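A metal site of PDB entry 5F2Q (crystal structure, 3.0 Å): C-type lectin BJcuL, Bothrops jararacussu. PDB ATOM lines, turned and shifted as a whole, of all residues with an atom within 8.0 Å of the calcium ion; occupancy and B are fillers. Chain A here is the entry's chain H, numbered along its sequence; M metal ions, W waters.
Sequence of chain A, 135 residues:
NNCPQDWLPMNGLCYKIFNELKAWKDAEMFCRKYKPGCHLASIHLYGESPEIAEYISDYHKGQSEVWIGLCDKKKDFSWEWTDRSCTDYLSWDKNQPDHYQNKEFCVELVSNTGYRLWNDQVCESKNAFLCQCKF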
ATOM      1  N   TRP A  92     -22.252  -5.249 -16.863  1.00  0.00           N
ATOM      2  CA  TRP A  92     -22.909  -3.997 -16.550  1.00  0.00           C
ATOM      3  C   TRP A  92     -24.399  -4.204 -16.315  1.00  0.00           C
ATOM      4  O   TRP A  92     -25.010  -5.156 -16.793  1.00  0.00           O
ATOM      5  CB  TRP A  92     -22.732  -2.978 -17.680  1.00  0.00           C
ATOM      6  CG  TRP A  92     -21.319  -2.650 -18.083  1.00  0.00           C
ATOM      7  CD1 TRP A  92     -20.590  -3.231 -19.081  1.00  0.00           C
ATOM      8  CD2 TRP A  92     -20.470  -1.654 -17.499  1.00  0.00           C
ATOM      9  NE1 TRP A  92     -19.347  -2.660 -19.159  1.00  0.00           N
ATOM     10  CE2 TRP A  92     -19.245  -1.690 -18.192  1.00  0.00           C
ATOM     11  CE3 TRP A  92     -20.621  -0.735 -16.454  1.00  0.00           C
ATOM     12  CZ2 TRP A  92     -18.181  -0.847 -17.885  1.00  0.00           C
ATOM     13  CZ3 TRP A  92     -19.565   0.105 -16.151  1.00  0.00           C
ATOM     14  CH2 TRP A  92     -18.356   0.038 -16.860  1.00  0.00           C
ATOM     15  N   LYS A  94     -28.388  -2.828 -16.781  1.00  0.00           N
ATOM     16  CA  LYS A  94     -29.099  -2.388 -17.964  1.00  0.00           C
ATOM     17  C   LYS A  94     -28.820  -0.915 -18.253  1.00  0.00           C
ATOM     18  O   LYS A  94     -28.907  -0.075 -17.356  1.00  0.00           O
ATOM     19  CB  LYS A  94     -30.609  -2.616 -17.809  1.00  0.00           C
ATOM     20  CG  LYS A  94     -31.073  -4.011 -18.228  1.00  0.00           C
ATOM     21  CD  LYS A  94     -32.602  -4.127 -18.275  1.00  0.00           C
ATOM     22  CE  LYS A  94     -33.216  -3.320 -19.420  1.00  0.00           C
ATOM     23  NZ  LYS A  94     -34.683  -3.550 -19.561  1.00  0.00           N
ATOM     24  N   ASN A  95     -28.475  -0.622 -19.507  1.00  0.00           N
ATOM     25  CA  ASN A  95     -28.197   0.743 -19.956  1.00  0.00           C
ATOM     26  C   ASN A  95     -26.981   1.347 -19.242  1.00  0.00           C
ATOM     27  O   ASN A  95     -26.936   2.556 -19.005  1.00  0.00           O
ATOM     28  CB  ASN A  95     -29.412   1.652 -19.786  1.00  0.00           C
ATOM     29  CG  ASN A  95     -30.594   1.197 -20.626  1.00  0.00           C
ATOM     30  OD1 ASN A  95     -30.420   0.645 -21.717  1.00  0.00           O
ATOM     31  ND2 ASN A  95     -31.793   1.434 -20.124  1.00  0.00           N
ATOM     32  N   GLN A  96     -26.013   0.506 -18.886  1.00  0.00           N
ATOM     33  CA  GLN A  96     -24.745   0.994 -18.357  1.00  0.00           C
ATOM     34  C   GLN A  96     -23.609   0.376 -19.185  1.00  0.00           C
ATOM     35  O   GLN A  96     -23.744  -0.744 -19.677  1.00  0.00           O
ATOM     36  CB  GLN A  96     -24.583   0.640 -16.879  1.00  0.00           C
ATOM     37  CG  GLN A  96     -25.656   1.234 -15.970  1.00  0.00           C
ATOM     38  CD  GLN A  96     -25.509   2.737 -15.760  1.00  0.00           C
ATOM     39  OE1 GLN A  96     -24.403   3.286 -15.814  1.00  0.00           O
ATOM     40  NE2 GLN A  96     -26.620   3.403 -15.514  1.00  0.00           N
ATOM     41  N   PRO A  97     -22.494   1.101 -19.364  1.00  0.00           N
ATOM     42  CA  PRO A  97     -22.192   2.446 -18.857  1.00  0.00           C
ATOM     43  C   PRO A  97     -23.014   3.505 -19.595  1.00  0.00           C
ATOM     44  O   PRO A  97     -23.776   3.153 -20.501  1.00  0.00           O
ATOM     45  CB  PRO A  97     -20.701   2.592 -19.116  1.00  0.00           C
ATOM     46  CG  PRO A  97     -20.447   1.752 -20.316  1.00  0.00           C
ATOM     47  CD  PRO A  97     -21.426   0.601 -20.245  1.00  0.00           C
ATOM     48  N   ASP A  98     -22.861   4.781 -19.229  1.00  0.00           N
ATOM     49  CA  ASP A  98     -23.774   5.801 -19.730  1.00  0.00           C
ATOM     50  C   ASP A  98     -23.198   7.213 -19.723  1.00  0.00           C
ATOM     51  O   ASP A  98     -23.897   8.159 -20.073  1.00  0.00           O
ATOM     52  CB  ASP A  98     -25.073   5.765 -18.915  1.00  0.00           C
ATOM     53  CG  ASP A  98     -24.854   6.112 -17.440  1.00  0.00           C
ATOM     54  OD1 ASP A  98     -24.076   7.041 -17.139  1.00  0.00           O
ATOM     55  OD2 ASP A  98     -25.459   5.451 -16.567  1.00  0.00           O
ATOM     56  N   HIS A  99     -21.915   7.349 -19.356  1.00  0.00           N
ATOM     57  CA  HIS A  99     -21.300   8.640 -19.025  1.00  0.00           C
ATOM     58  C   HIS A  99     -22.320   9.742 -18.758  1.00  0.00           C
ATOM     59  O   HIS A  99     -22.517  10.640 -19.584  1.00  0.00           O
ATOM     60  CB  HIS A  99     -20.322   9.072 -20.121  1.00  0.00           C
ATOM     61  CG  HIS A  99     -18.996   8.380 -20.035  1.00  0.00           C
ATOM     62  ND1 HIS A  99     -17.899   8.775 -20.772  1.00  0.00           N
ATOM     63  CD2 HIS A  99     -18.579   7.335 -19.280  1.00  0.00           C
ATOM     64  CE1 HIS A  99     -16.869   7.999 -20.485  1.00  0.00           C
ATOM     65  NE2 HIS A  99     -17.261   7.113 -19.590  1.00  0.00           N
ATOM     66  N   TYR A 100     -22.972   9.673 -17.598  1.00  0.00           N
ATOM     67  CA  TYR A 100     -23.914  10.684 -17.143  1.00  0.00           C
ATOM     68  C   TYR A 100     -23.158  11.959 -16.791  1.00  0.00           C
ATOM     69  O   TYR A 100     -23.130  12.363 -15.629  1.00  0.00           O
ATOM     70  CB  TYR A 100     -24.683  10.143 -15.930  1.00  0.00           C
ATOM     71  CG  TYR A 100     -26.032  10.765 -15.658  1.00  0.00           C
ATOM     72  CD1 TYR A 100     -27.155  10.368 -16.364  1.00  0.00           C
ATOM     73  CD2 TYR A 100     -26.185  11.713 -14.655  1.00  0.00           C
ATOM     74  CE1 TYR A 100     -28.396  10.924 -16.106  1.00  0.00           C
ATOM     75  CE2 TYR A 100     -27.423  12.273 -14.384  1.00  0.00           C
ATOM     76  CZ  TYR A 100     -28.521  11.874 -15.110  1.00  0.00           C
ATOM     77  OH  TYR A 100     -29.753  12.424 -14.845  1.00  0.00           O
ATOM     78  N   GLU A 104     -18.690  10.950 -13.958  1.00  0.00           N
ATOM     79  CA  GLU A 104     -18.880   9.498 -13.953  1.00  0.00           C
ATOM     80  C   GLU A 104     -17.803   8.813 -14.781  1.00  0.00           C
ATOM     81  O   GLU A 104     -17.920   8.681 -16.005  1.00  0.00           O
ATOM     82  CB  GLU A 104     -20.260   9.139 -14.505  1.00  0.00           C
ATOM     83  CG  GLU A 104     -21.413   9.418 -13.550  1.00  0.00           C
ATOM     84  CD  GLU A 104     -22.624   8.552 -13.861  1.00  0.00           C
ATOM     85  OE1 GLU A 104     -23.408   8.258 -12.933  1.00  0.00           O
ATOM     86  OE2 GLU A 104     -22.798   8.165 -15.036  1.00  0.00           O
ATOM     87  N   CYS A 106     -15.787   6.050 -12.872  1.00  0.00           N
ATOM     88  CA  CYS A 106     -15.383   4.931 -12.039  1.00  0.00           C
ATOM     89  C   CYS A 106     -16.549   3.960 -11.918  1.00  0.00           C
ATOM     90  O   CYS A 106     -17.714   4.349 -12.048  1.00  0.00           O
ATOM     91  CB  CYS A 106     -14.931   5.395 -10.656  1.00  0.00           C
ATOM     92  SG  CYS A 106     -13.530   6.527 -10.707  1.00  0.00           S
ATOM     93  N   GLU A 108     -18.790   0.853 -10.000  1.00  0.00           N
ATOM     94  CA  GLU A 108     -19.249   0.402  -8.692  1.00  0.00           C
ATOM     95  C   GLU A 108     -20.159  -0.811  -8.853  1.00  0.00           C
ATOM     96  O   GLU A 108     -20.664  -1.094  -9.946  1.00  0.00           O
ATOM     97  CB  GLU A 108     -19.997   1.521  -7.943  1.00  0.00           C
ATOM     98  CG  GLU A 108     -21.203   2.064  -8.681  1.00  0.00           C
ATOM     99  CD  GLU A 108     -21.917   3.173  -7.920  1.00  0.00           C
ATOM    100  OE1 GLU A 108     -21.476   3.506  -6.794  1.00  0.00           O
ATOM    101  OE2 GLU A 108     -22.913   3.706  -8.439  1.00  0.00           O
ATOM    102  N   TRP A 118     -22.530  -3.932 -12.796  1.00  0.00           N
ATOM    103  CA  TRP A 118     -21.681  -2.764 -12.665  1.00  0.00           C
ATOM    104  C   TRP A 118     -22.425  -1.483 -13.049  1.00  0.00           C
ATOM    105  O   TRP A 118     -23.439  -1.513 -13.758  1.00  0.00           O
ATOM    106  CB  TRP A 118     -20.424  -2.915 -13.531  1.00  0.00           C
ATOM    107  CG  TRP A 118     -19.601  -4.133 -13.205  1.00  0.00           C
ATOM    108  CD1 TRP A 118     -19.700  -4.912 -12.085  1.00  0.00           C
ATOM    109  CD2 TRP A 118     -18.574  -4.724 -14.011  1.00  0.00           C
ATOM    110  NE1 TRP A 118     -18.785  -5.947 -12.145  1.00  0.00           N
ATOM    111  CE2 TRP A 118     -18.081  -5.848 -13.313  1.00  0.00           C
ATOM    112  CE3 TRP A 118     -18.006  -4.399 -15.250  1.00  0.00           C
ATOM    113  CZ2 TRP A 118     -17.063  -6.644 -13.822  1.00  0.00           C
ATOM    114  CZ3 TRP A 118     -17.002  -5.197 -15.755  1.00  0.00           C
ATOM    115  CH2 TRP A 118     -16.535  -6.309 -15.040  1.00  0.00           C
ATOM    116  N   ASN A 119     -21.891  -0.359 -12.581  1.00  0.00           N
ATOM    117  CA  ASN A 119     -22.426   0.961 -12.888  1.00  0.00           C
ATOM    118  C   ASN A 119     -21.295   1.975 -12.824  1.00  0.00           C
ATOM    119  O   ASN A 119     -20.436   1.895 -11.952  1.00  0.00           O
ATOM    120  CB  ASN A 119     -23.532   1.375 -11.918  1.00  0.00           C
ATOM    121  CG  ASN A 119     -23.942   2.822 -12.086  1.00  0.00           C
ATOM    122  OD1 ASN A 119     -24.226   3.273 -13.193  1.00  0.00           O
ATOM    123  ND2 ASN A 119     -23.947   3.575 -10.987  1.00  0.00           N
ATOM    124  N   ASP A 120     -21.314   2.932 -13.753  1.00  0.00           N
ATOM    125  CA  ASP A 120     -20.390   4.051 -13.721  1.00  0.00           C
ATOM    126  C   ASP A 120     -20.995   5.197 -12.923  1.00  0.00           C
ATOM    127  O   ASP A 120     -22.143   5.591 -13.175  1.00  0.00           O
ATOM    128  CB  ASP A 120     -20.029   4.498 -15.138  1.00  0.00           C
ATOM    129  CG  ASP A 120     -21.248   4.929 -15.946  1.00  0.00           C
ATOM    130  OD1 ASP A 120     -22.386   4.637 -15.518  1.00  0.00           O
ATOM    131  OD2 ASP A 120     -21.068   5.551 -17.008  1.00  0.00           O
ATOM    132  N   GLN A 121     -20.235   5.726 -11.968  1.00  0.00           N
ATOM    133  CA  GLN A 121     -20.703   6.788 -11.091  1.00  0.00           C
ATOM    134  C   GLN A 121     -19.560   7.755 -10.819  1.00  0.00           C
ATOM    135  O   GLN A 121     -18.391   7.477 -11.104  1.00  0.00           O
ATOM    136  CB  GLN A 121     -21.260   6.225  -9.763  1.00  0.00           C
ATOM    137  CG  GLN A 121     -21.777   7.284  -8.797  1.00  0.00           C
ATOM    138  CD  GLN A 121     -22.683   6.723  -7.715  1.00  0.00           C
ATOM    139  OE1 GLN A 121     -22.216   6.156  -6.721  1.00  0.00           O
ATOM    140  NE2 GLN A 121     -23.990   6.879  -7.901  1.00  0.00           N
ATOM    141  N   VAL A 122     -19.906   8.912 -10.254  1.00  0.00           N
ATOM    142  CA  VAL A 122     -18.933   9.971 -10.048  1.00  0.00           C
ATOM    143  C   VAL A 122     -17.782   9.486  -9.164  1.00  0.00           C
ATOM    144  O   VAL A 122     -17.990   8.797  -8.155  1.00  0.00           O
ATOM    145  CB  VAL A 122     -19.613  11.217  -9.448  1.00  0.00           C
ATOM    146  CG1 VAL A 122     -20.741  11.683 -10.337  1.00  0.00           C
ATOM    147  CG2 VAL A 122     -20.111  10.940  -8.043  1.00  0.00           C
HETATM  148 CA    CA M   1     -24.317   5.350 -14.397  1.00  0.00          CA
HETATM  149  O   HOH W   1     -25.040   6.418 -12.363  1.00  0.00           O
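OD2 of Asp 120 lies within hydrogen-bond range of N of His 99, 3.1 Å away.
The side-chain carboxylate of Asp 98 is in hydrogen-bond range of the backbone NH of Tyr 100, at 2.9 Å.
OD1 of Asp 98 lies close to OE2 of Glu 104, at 2.7 Å.
The side-chain carboxylate (OE2) of Glu 104 lies close to the backbone NH (N) of Tyr 100 (3.0 Å).
The side-chain carboxylate (OE2) of Glu 108 sits at hydrogen-bond distance from the side-chain amide nitrogen (ND2) of Asn 119, at 2.8 Å.
Merely in contact with the calcium ion: Glu 104 (3.3 Å).
Within 4 Å of the calcium ion: Gln 96, Asp 98, Glu 104, Asn 119 and Asp 120.
Along chain A the residues within 4 Å of the calcium ion span positions 96 to 120.
The calcium ion is bound by OD1 of Asp 120, OD1 of Asn 119, water W1, OD2 of Asp 98, O of Asp 120 and OE1 of Gln 96.
Water W1 bridges OE1 of Glu 104 (2.5 Å) and ND2 of Asn 119 (3.3 Å).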
